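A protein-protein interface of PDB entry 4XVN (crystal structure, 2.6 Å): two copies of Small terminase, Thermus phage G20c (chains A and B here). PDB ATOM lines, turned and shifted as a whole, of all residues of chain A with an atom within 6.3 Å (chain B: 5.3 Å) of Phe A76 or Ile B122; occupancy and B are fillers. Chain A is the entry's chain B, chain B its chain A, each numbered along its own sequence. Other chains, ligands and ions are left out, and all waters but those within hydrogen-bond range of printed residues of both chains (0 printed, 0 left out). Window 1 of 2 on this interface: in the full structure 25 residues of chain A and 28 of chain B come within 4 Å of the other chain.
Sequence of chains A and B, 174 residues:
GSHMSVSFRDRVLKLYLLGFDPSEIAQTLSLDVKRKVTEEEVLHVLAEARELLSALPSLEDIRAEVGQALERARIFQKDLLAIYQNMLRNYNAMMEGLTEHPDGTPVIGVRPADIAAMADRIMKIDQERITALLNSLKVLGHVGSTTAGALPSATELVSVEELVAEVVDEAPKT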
ATOM      1  N   GLU A  71       4.063  -3.522  -7.615  1.00  0.00           N
ATOM      2  CA  GLU A  71       2.984  -3.312  -6.644  1.00  0.00           C
ATOM      3  C   GLU A  71       3.429  -2.367  -5.525  1.00  0.00           C
ATOM      4  O   GLU A  71       2.649  -1.522  -5.079  1.00  0.00           O
ATOM      5  CB  GLU A  71       2.511  -4.649  -6.057  1.00  0.00           C
ATOM      6  CG  GLU A  71       1.221  -4.578  -5.242  1.00  0.00           C
ATOM      7  CD  GLU A  71       0.021  -4.076  -6.036  1.00  0.00           C
ATOM      8  OE1 GLU A  71      -0.063  -4.351  -7.254  1.00  0.00           O
ATOM      9  OE2 GLU A  71      -0.845  -3.405  -5.433  1.00  0.00           O
ATOM     10  N   ARG A  72       4.675  -2.521  -5.072  1.00  0.00           N
ATOM     11  CA  ARG A  72       5.290  -1.576  -4.127  1.00  0.00           C
ATOM     12  C   ARG A  72       5.391  -0.163  -4.723  1.00  0.00           C
ATOM     13  O   ARG A  72       5.206   0.825  -4.011  1.00  0.00           O
ATOM     14  CB  ARG A  72       6.671  -2.078  -3.669  1.00  0.00           C
ATOM     15  CG  ARG A  72       7.500  -1.059  -2.895  1.00  0.00           C
ATOM     16  CD  ARG A  72       8.619  -1.686  -2.074  1.00  0.00           C
ATOM     17  NE  ARG A  72       9.302  -2.782  -2.773  1.00  0.00           N
ATOM     18  CZ  ARG A  72       9.359  -4.061  -2.381  1.00  0.00           C
ATOM     19  NH1 ARG A  72       8.779  -4.490  -1.257  1.00  0.00           N
ATOM     20  NH2 ARG A  72      10.023  -4.937  -3.132  1.00  0.00           N
ATOM     21  N   ALA A  73       5.686  -0.078  -6.020  1.00  0.00           N
ATOM     22  CA  ALA A  73       5.716   1.203  -6.735  1.00  0.00           C
ATOM     23  C   ALA A  73       4.347   1.888  -6.751  1.00  0.00           C
ATOM     24  O   ALA A  73       4.262   3.103  -6.565  1.00  0.00           O
ATOM     25  CB  ALA A  73       6.230   1.011  -8.155  1.00  0.00           C
ATOM     26  N   ARG A  74       3.287   1.110  -6.968  1.00  0.00           N
ATOM     27  CA  ARG A  74       1.913   1.630  -6.923  1.00  0.00           C
ATOM     28  C   ARG A  74       1.526   2.165  -5.541  1.00  0.00           C
ATOM     29  O   ARG A  74       0.776   3.139  -5.448  1.00  0.00           O
ATOM     30  CB  ARG A  74       0.905   0.560  -7.361  1.00  0.00           C
ATOM     31  CG  ARG A  74       0.923   0.252  -8.849  1.00  0.00           C
ATOM     32  CD  ARG A  74       0.000  -0.913  -9.174  1.00  0.00           C
ATOM     33  NE  ARG A  74       0.191  -1.423 -10.534  1.00  0.00           N
ATOM     34  CZ  ARG A  74      -0.265  -0.852 -11.653  1.00  0.00           C
ATOM     35  NH1 ARG A  74      -0.952   0.291 -11.625  1.00  0.00           N
ATOM     36  NH2 ARG A  74      -0.020  -1.433 -12.825  1.00  0.00           N
ATOM     37  N   ILE A  75       2.029   1.524  -4.483  1.00  0.00           N
ATOM     38  CA  ILE A  75       1.809   1.984  -3.102  1.00  0.00           C
ATOM     39  C   ILE A  75       2.479   3.343  -2.871  1.00  0.00           C
ATOM     40  O   ILE A  75       1.867   4.243  -2.294  1.00  0.00           O
ATOM     41  CB  ILE A  75       2.309   0.950  -2.059  1.00  0.00           C
ATOM     42  CG1 ILE A  75       1.436  -0.310  -2.106  1.00  0.00           C
ATOM     43  CG2 ILE A  75       2.294   1.531  -0.643  1.00  0.00           C
ATOM     44  CD1 ILE A  75       2.057  -1.524  -1.449  1.00  0.00           C
ATOM     45  N   PHE A  76       3.730   3.478  -3.313  1.00  0.00           N
ATOM     46  CA  PHE A  76       4.441   4.756  -3.241  1.00  0.00           C
ATOM     47  C   PHE A  76       3.751   5.811  -4.100  1.00  0.00           C
ATOM     48  O   PHE A  76       3.550   6.938  -3.653  1.00  0.00           O
ATOM     49  CB  PHE A  76       5.903   4.622  -3.697  1.00  0.00           C
ATOM     50  CG  PHE A  76       6.784   3.830  -2.760  1.00  0.00           C
ATOM     51  CD1 PHE A  76       6.796   4.083  -1.391  1.00  0.00           C
ATOM     52  CD2 PHE A  76       7.645   2.858  -3.259  1.00  0.00           C
ATOM     53  CE1 PHE A  76       7.620   3.362  -0.538  1.00  0.00           C
ATOM     54  CE2 PHE A  76       8.472   2.136  -2.411  1.00  0.00           C
ATOM     55  CZ  PHE A  76       8.461   2.388  -1.050  1.00  0.00           C
ATOM     56  N   GLN A  77       3.384   5.433  -5.324  1.00  0.00           N
ATOM     57  CA  GLN A  77       2.685   6.332  -6.252  1.00  0.00           C
ATOM     58  C   GLN A  77       1.370   6.858  -5.673  1.00  0.00           C
ATOM     59  O   GLN A  77       1.028   8.022  -5.877  1.00  0.00           O
ATOM     60  CB  GLN A  77       2.426   5.631  -7.592  1.00  0.00           C
ATOM     61  CG  GLN A  77       1.973   6.560  -8.709  1.00  0.00           C
ATOM     62  CD  GLN A  77       1.934   5.871 -10.062  1.00  0.00           C
ATOM     63  OE1 GLN A  77       1.488   4.728 -10.177  1.00  0.00           O
ATOM     64  NE2 GLN A  77       2.396   6.566 -11.095  1.00  0.00           N
ATOM     65  N   LYS A  78       0.650   6.003  -4.951  1.00  0.00           N
ATOM     66  CA  LYS A  78      -0.590   6.399  -4.279  1.00  0.00           C
ATOM     67  C   LYS A  78      -0.327   7.358  -3.108  1.00  0.00           C
ATOM     68  O   LYS A  78      -1.109   8.287  -2.881  1.00  0.00           O
ATOM     69  CB  LYS A  78      -1.354   5.163  -3.798  1.00  0.00           C
ATOM     70  CG  LYS A  78      -2.808   5.428  -3.448  1.00  0.00           C
ATOM     71  CD  LYS A  78      -3.549   4.126  -3.185  1.00  0.00           C
ATOM     72  CE  LYS A  78      -5.019   4.364  -2.877  1.00  0.00           C
ATOM     73  NZ  LYS A  78      -5.224   5.182  -1.648  1.00  0.00           N
ATOM     74  N   ASP A  79       0.765   7.131  -2.374  1.00  0.00           N
ATOM     75  CA  ASP A  79       1.193   8.044  -1.303  1.00  0.00           C
ATOM     76  C   ASP A  79       1.604   9.421  -1.845  1.00  0.00           C
ATOM     77  O   ASP A  79       1.228  10.446  -1.276  1.00  0.00           O
ATOM     78  CB  ASP A  79       2.354   7.446  -0.486  1.00  0.00           C
ATOM     79  CG  ASP A  79       1.941   6.243   0.364  1.00  0.00           C
ATOM     80  OD1 ASP A  79       0.728   5.980   0.535  1.00  0.00           O
ATOM     81  OD2 ASP A  79       2.851   5.558   0.880  1.00  0.00           O
ATOM     82  N   LEU A  80       2.371   9.439  -2.937  1.00  0.00           N
ATOM     83  CA  LEU A  80       2.822  10.695  -3.553  1.00  0.00           C
ATOM     84  C   LEU A  80       1.687  11.485  -4.206  1.00  0.00           C
ATOM     85  O   LEU A  80       1.717  12.718  -4.206  1.00  0.00           O
ATOM     86  CB  LEU A  80       3.934  10.438  -4.581  1.00  0.00           C
ATOM     87  CG  LEU A  80       5.258   9.848  -4.076  1.00  0.00           C
ATOM     88  CD1 LEU A  80       6.219   9.666  -5.239  1.00  0.00           C
ATOM     89  CD2 LEU A  80       5.901  10.700  -2.990  1.00  0.00           C
ATOM     90  N   LEU A  81       0.703  10.781  -4.769  1.00  0.00           N
ATOM     91  CA  LEU A  81      -0.512  11.419  -5.294  1.00  0.00           C
ATOM     92  C   LEU A  81      -1.318  12.116  -4.194  1.00  0.00           C
ATOM     93  O   LEU A  81      -1.847  13.203  -4.411  1.00  0.00           O
ATOM     94  CB  LEU A  81      -1.395  10.407  -6.035  1.00  0.00           C
ATOM     95  CG  LEU A  81      -0.915  10.041  -7.446  1.00  0.00           C
ATOM     96  CD1 LEU A  81      -1.483   8.706  -7.907  1.00  0.00           C
ATOM     97  CD2 LEU A  81      -1.264  11.136  -8.444  1.00  0.00           C
ATOM     98  N   ILE A 125       7.275   7.086 -12.305  1.00  0.00           N
ATOM     99  CA  ILE A 125       6.878   5.761 -11.803  1.00  0.00           C
ATOM    100  C   ILE A 125       6.075   4.989 -12.861  1.00  0.00           C
ATOM    101  O   ILE A 125       6.192   3.767 -12.949  1.00  0.00           O
ATOM    102  CB  ILE A 125       6.098   5.852 -10.466  1.00  0.00           C
ATOM    103  CG1 ILE A 125       7.012   6.403  -9.361  1.00  0.00           C
ATOM    104  CG2 ILE A 125       5.564   4.486 -10.034  1.00  0.00           C
ATOM    105  CD1 ILE A 125       6.275   6.925  -8.143  1.00  0.00           C
ATOM    106  N   GLN B  77      17.193  -2.174   1.840  1.00  0.00           N
ATOM    107  CA  GLN B  77      15.833  -1.760   1.476  1.00  0.00           C
ATOM    108  C   GLN B  77      14.875  -1.788   2.671  1.00  0.00           C
ATOM    109  O   GLN B  77      14.046  -0.890   2.809  1.00  0.00           O
ATOM    110  CB  GLN B  77      15.277  -2.608   0.327  1.00  0.00           C
ATOM    111  CG  GLN B  77      14.053  -2.001  -0.341  1.00  0.00           C
ATOM    112  CD  GLN B  77      13.631  -2.757  -1.585  1.00  0.00           C
ATOM    113  OE1 GLN B  77      13.421  -3.968  -1.546  1.00  0.00           O
ATOM    114  NE2 GLN B  77      13.499  -2.045  -2.697  1.00  0.00           N
ATOM    115  N   LEU B  80      15.633   1.249   4.888  1.00  0.00           N
ATOM    116  CA  LEU B  80      15.061   2.469   4.299  1.00  0.00           C
ATOM    117  C   LEU B  80      13.531   2.467   4.293  1.00  0.00           C
ATOM    118  O   LEU B  80      12.915   3.523   4.457  1.00  0.00           O
ATOM    119  CB  LEU B  80      15.595   2.689   2.879  1.00  0.00           C
ATOM    120  CG  LEU B  80      17.116   2.854   2.751  1.00  0.00           C
ATOM    121  CD1 LEU B  80      17.519   2.930   1.288  1.00  0.00           C
ATOM    122  CD2 LEU B  80      17.620   4.072   3.507  1.00  0.00           C
ATOM    123  N   LEU B  81      12.926   1.294   4.100  1.00  0.00           N
ATOM    124  CA  LEU B  81      11.464   1.141   4.191  1.00  0.00           C
ATOM    125  C   LEU B  81      10.917   1.525   5.568  1.00  0.00           C
ATOM    126  O   LEU B  81       9.848   2.130   5.663  1.00  0.00           O
ATOM    127  CB  LEU B  81      11.037  -0.291   3.844  1.00  0.00           C
ATOM    128  CG  LEU B  81      10.919  -0.624   2.352  1.00  0.00           C
ATOM    129  CD1 LEU B  81      10.934  -2.131   2.141  1.00  0.00           C
ATOM    130  CD2 LEU B  81       9.667  -0.008   1.743  1.00  0.00           C
ATOM    131  N   TYR B  84      11.142   5.289   5.735  1.00  0.00           N
ATOM    132  CA  TYR B  84      10.056   5.860   4.926  1.00  0.00           C
ATOM    133  C   TYR B  84       8.740   5.975   5.700  1.00  0.00           C
ATOM    134  O   TYR B  84       8.054   6.994   5.607  1.00  0.00           O
ATOM    135  CB  TYR B  84       9.832   5.028   3.655  1.00  0.00           C
ATOM    136  CG  TYR B  84       8.683   5.510   2.793  1.00  0.00           C
ATOM    137  CD1 TYR B  84       8.864   6.531   1.862  1.00  0.00           C
ATOM    138  CD2 TYR B  84       7.409   4.946   2.911  1.00  0.00           C
ATOM    139  CE1 TYR B  84       7.814   6.978   1.072  1.00  0.00           C
ATOM    140  CE2 TYR B  84       6.352   5.390   2.128  1.00  0.00           C
ATOM    141  CZ  TYR B  84       6.559   6.406   1.211  1.00  0.00           C
ATOM    142  OH  TYR B  84       5.517   6.846   0.427  1.00  0.00           O
ATOM    143  N   MET B 118      13.136   9.657  -0.850  1.00  0.00           N
ATOM    144  CA  MET B 118      13.311   8.379  -0.143  1.00  0.00           C
ATOM    145  C   MET B 118      12.592   7.255  -0.838  1.00  0.00           C
ATOM    146  O   MET B 118      13.095   6.133  -0.882  1.00  0.00           O
ATOM    147  CB  MET B 118      12.800   8.504   1.295  1.00  0.00           C
ATOM    148  CG  MET B 118      12.966   7.242   2.146  1.00  0.00           C
ATOM    149  SD  MET B 118      14.844   6.649   2.176  1.00  0.00           S
ATOM    150  CE  MET B 118      15.581   8.176   3.178  1.00  0.00           C
ATOM    151  N   ALA B 119      11.402   7.542  -1.364  1.00  0.00           N
ATOM    152  CA  ALA B 119      10.647   6.574  -2.161  1.00  0.00           C
ATOM    153  C   ALA B 119      11.410   6.155  -3.416  1.00  0.00           C
ATOM    154  O   ALA B 119      11.452   4.971  -3.748  1.00  0.00           O
ATOM    155  CB  ALA B 119       9.289   7.146  -2.541  1.00  0.00           C
ATOM    156  N   ASP B 120      12.009   7.130  -4.100  1.00  0.00           N
ATOM    157  CA  ASP B 120      12.779   6.876  -5.325  1.00  0.00           C
ATOM    158  C   ASP B 120      13.981   5.958  -5.086  1.00  0.00           C
ATOM    159  O   ASP B 120      14.239   5.060  -5.886  1.00  0.00           O
ATOM    160  CB  ASP B 120      13.246   8.199  -5.947  1.00  0.00           C
ATOM    161  CG  ASP B 120      13.970   8.006  -7.271  1.00  0.00           C
ATOM    162  OD1 ASP B 120      13.493   7.215  -8.115  1.00  0.00           O
ATOM    163  OD2 ASP B 120      15.021   8.655  -7.471  1.00  0.00           O
ATOM    164  N   ARG B 121      14.703   6.189  -3.991  1.00  0.00           N
ATOM    165  CA  ARG B 121      15.848   5.349  -3.619  1.00  0.00           C
ATOM    166  C   ARG B 121      15.449   3.901  -3.315  1.00  0.00           C
ATOM    167  O   ARG B 121      16.200   2.976  -3.627  1.00  0.00           O
ATOM    168  CB  ARG B 121      16.601   5.948  -2.427  1.00  0.00           C
ATOM    169  CG  ARG B 121      17.374   7.214  -2.768  1.00  0.00           C
ATOM    170  CD  ARG B 121      18.257   7.642  -1.610  1.00  0.00           C
ATOM    171  NE  ARG B 121      19.215   8.688  -1.968  1.00  0.00           N
ATOM    172  CZ  ARG B 121      20.350   8.501  -2.649  1.00  0.00           C
ATOM    173  NH1 ARG B 121      20.706   7.293  -3.095  1.00  0.00           N
ATOM    174  NH2 ARG B 121      21.140   9.542  -2.901  1.00  0.00           N
ATOM    175  N   ILE B 122      14.275   3.713  -2.713  1.00  0.00           N
ATOM    176  CA  ILE B 122      13.729   2.376  -2.458  1.00  0.00           C
ATOM    177  C   ILE B 122      13.356   1.685  -3.778  1.00  0.00           C
ATOM    178  O   ILE B 122      13.624   0.493  -3.953  1.00  0.00           O
ATOM    179  CB  ILE B 122      12.510   2.428  -1.497  1.00  0.00           C
ATOM    180  CG1 ILE B 122      12.950   2.907  -0.104  1.00  0.00           C
ATOM    181  CG2 ILE B 122      11.841   1.061  -1.372  1.00  0.00           C
ATOM    182  CD1 ILE B 122      11.824   3.442   0.756  1.00  0.00           C
ATOM    183  N   MET B 123      12.745   2.435  -4.696  1.00  0.00           N
ATOM    184  CA  MET B 123      12.366   1.909  -6.016  1.00  0.00           C
ATOM    185  C   MET B 123      13.560   1.680  -6.913  1.00  0.00           C
ATOM    186  O   MET B 123      13.525   0.780  -7.754  1.00  0.00           O
ATOM    187  CB  MET B 123      11.356   2.831  -6.701  1.00  0.00           C
ATOM    188  CG  MET B 123      10.009   2.777  -5.985  1.00  0.00           C
ATOM    189  SD  MET B 123       8.671   3.932  -6.860  1.00  0.00           S
ATOM    190  CE  MET B 123       9.582   5.677  -6.818  1.00  0.00           C
ATOM    191  N   LYS B 124      14.615   2.485  -6.757  1.00  0.00           N
ATOM    192  CA  LYS B 124      15.883   2.267  -7.475  1.00  0.00           C
ATOM    193  C   LYS B 124      16.496   0.899  -7.174  1.00  0.00           C
ATOM    194  O   LYS B 124      17.029   0.253  -8.074  1.00  0.00           O
ATOM    195  CB  LYS B 124      16.906   3.364  -7.148  1.00  0.00           C
ATOM    196  CG  LYS B 124      16.706   4.656  -7.924  1.00  0.00           C
ATOM    197  CD  LYS B 124      17.259   4.565  -9.338  1.00  0.00           C
ATOM    198  CE  LYS B 124      17.097   5.885 -10.075  1.00  0.00           C
ATOM    199  NZ  LYS B 124      17.581   5.809 -11.481  1.00  0.00           N
ATOM    200  N   ILE B 125      16.414   0.473  -5.914  1.00  0.00           N
ATOM    201  CA  ILE B 125      16.917  -0.841  -5.488  1.00  0.00           C
ATOM    202  C   ILE B 125      16.156  -1.971  -6.191  1.00  0.00           C
ATOM    203  O   ILE B 125      16.765  -2.958  -6.612  1.00  0.00           O
ATOM    204  CB  ILE B 125      16.846  -1.012  -3.946  1.00  0.00           C
ATOM    205  CG1 ILE B 125      17.816  -0.043  -3.256  1.00  0.00           C
ATOM    206  CG2 ILE B 125      17.167  -2.447  -3.525  1.00  0.00           C
ATOM    207  CD1 ILE B 125      17.531   0.186  -1.786  1.00  0.00           C
ATOM    208  N   ASP B 126      14.836  -1.819  -6.313  1.00  0.00           N
ATOM    209  CA  ASP B 126      13.998  -2.789  -7.030  1.00  0.00           C
ATOM    210  C   ASP B 126      14.312  -2.855  -8.528  1.00  0.00           C
ATOM    211  O   ASP B 126      14.315  -3.941  -9.106  1.00  0.00           O
ATOM    212  CB  ASP B 126      12.506  -2.480  -6.834  1.00  0.00           C
ATOM    213  CG  ASP B 126      12.028  -2.747  -5.416  1.00  0.00           C
ATOM    214  OD1 ASP B 126      12.407  -3.784  -4.829  1.00  0.00           O
ATOM    215  OD2 ASP B 126      11.256  -1.921  -4.888  1.00  0.00           O
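NE2 of Gln B77 sits at hydrogen-bond distance from O of Ile B122, at 2.8 Å. NE2 of Gln B77 is in hydrogen-bond range of OD1 of Asp B126 (3.0 Å).
Phe A76 touches just these residues of chain B: Leu B81 (3.9 Å), Tyr B84 (3.5 Å), Ile B122 (3.6 Å) and Met B123 (3.6 Å). Ile B122 touches one residue of chain A. Printed residues of chain A within 4 Å of Leu B81: Phe A76 (3.9 Å). Of the printed residues of chain A, Gln B77 touches Arg A72 (3.9 Å). Lys B124 touches none of the printed residues of chain A. The nearest residue of chain B that does not touch Phe A76 is Ala B119 (4.1 Å). The nearest printed residue of chain A that does not touch Met B123 is Ala A73 (4.02 Å).
The side-chain hydroxyl of Tyr B84 is in hydrogen-bond range of the side-chain carboxylate of Asp A79. The side-chain carboxylate (OD2) of Asp B126 is in salt-bridge range of the guanidinium group (NE) of Arg A72, at 3.0 Å.
Among the printed residues, pairs that only touch across the chains: Phe A76 with Tyr B84, Phe A76 with Met B123, Phe A76 with Ile B122, Ile A125 with Met B123, Phe A76 with Leu B81 and Arg A72 with Gln B77.
Along chain A the printed residues that touch a printed residue of chain B span positions 72 to 125. Of the 13 printed residues of chain B, 6 touch a printed residue of chain A. Among the printed residues, 8 pairs touch across the chains. Among the printed residues, Asp or Glu carboxylates within 4 Å of a Lys or Arg side-chain nitrogen of the other chain: Arg A72 with Asp B126 (3.0 Å).
4 positions are printed for both chains. Of the 8 pairs that touch across the chains among the printed residues, none has its exchanged pair printed and touching as well.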
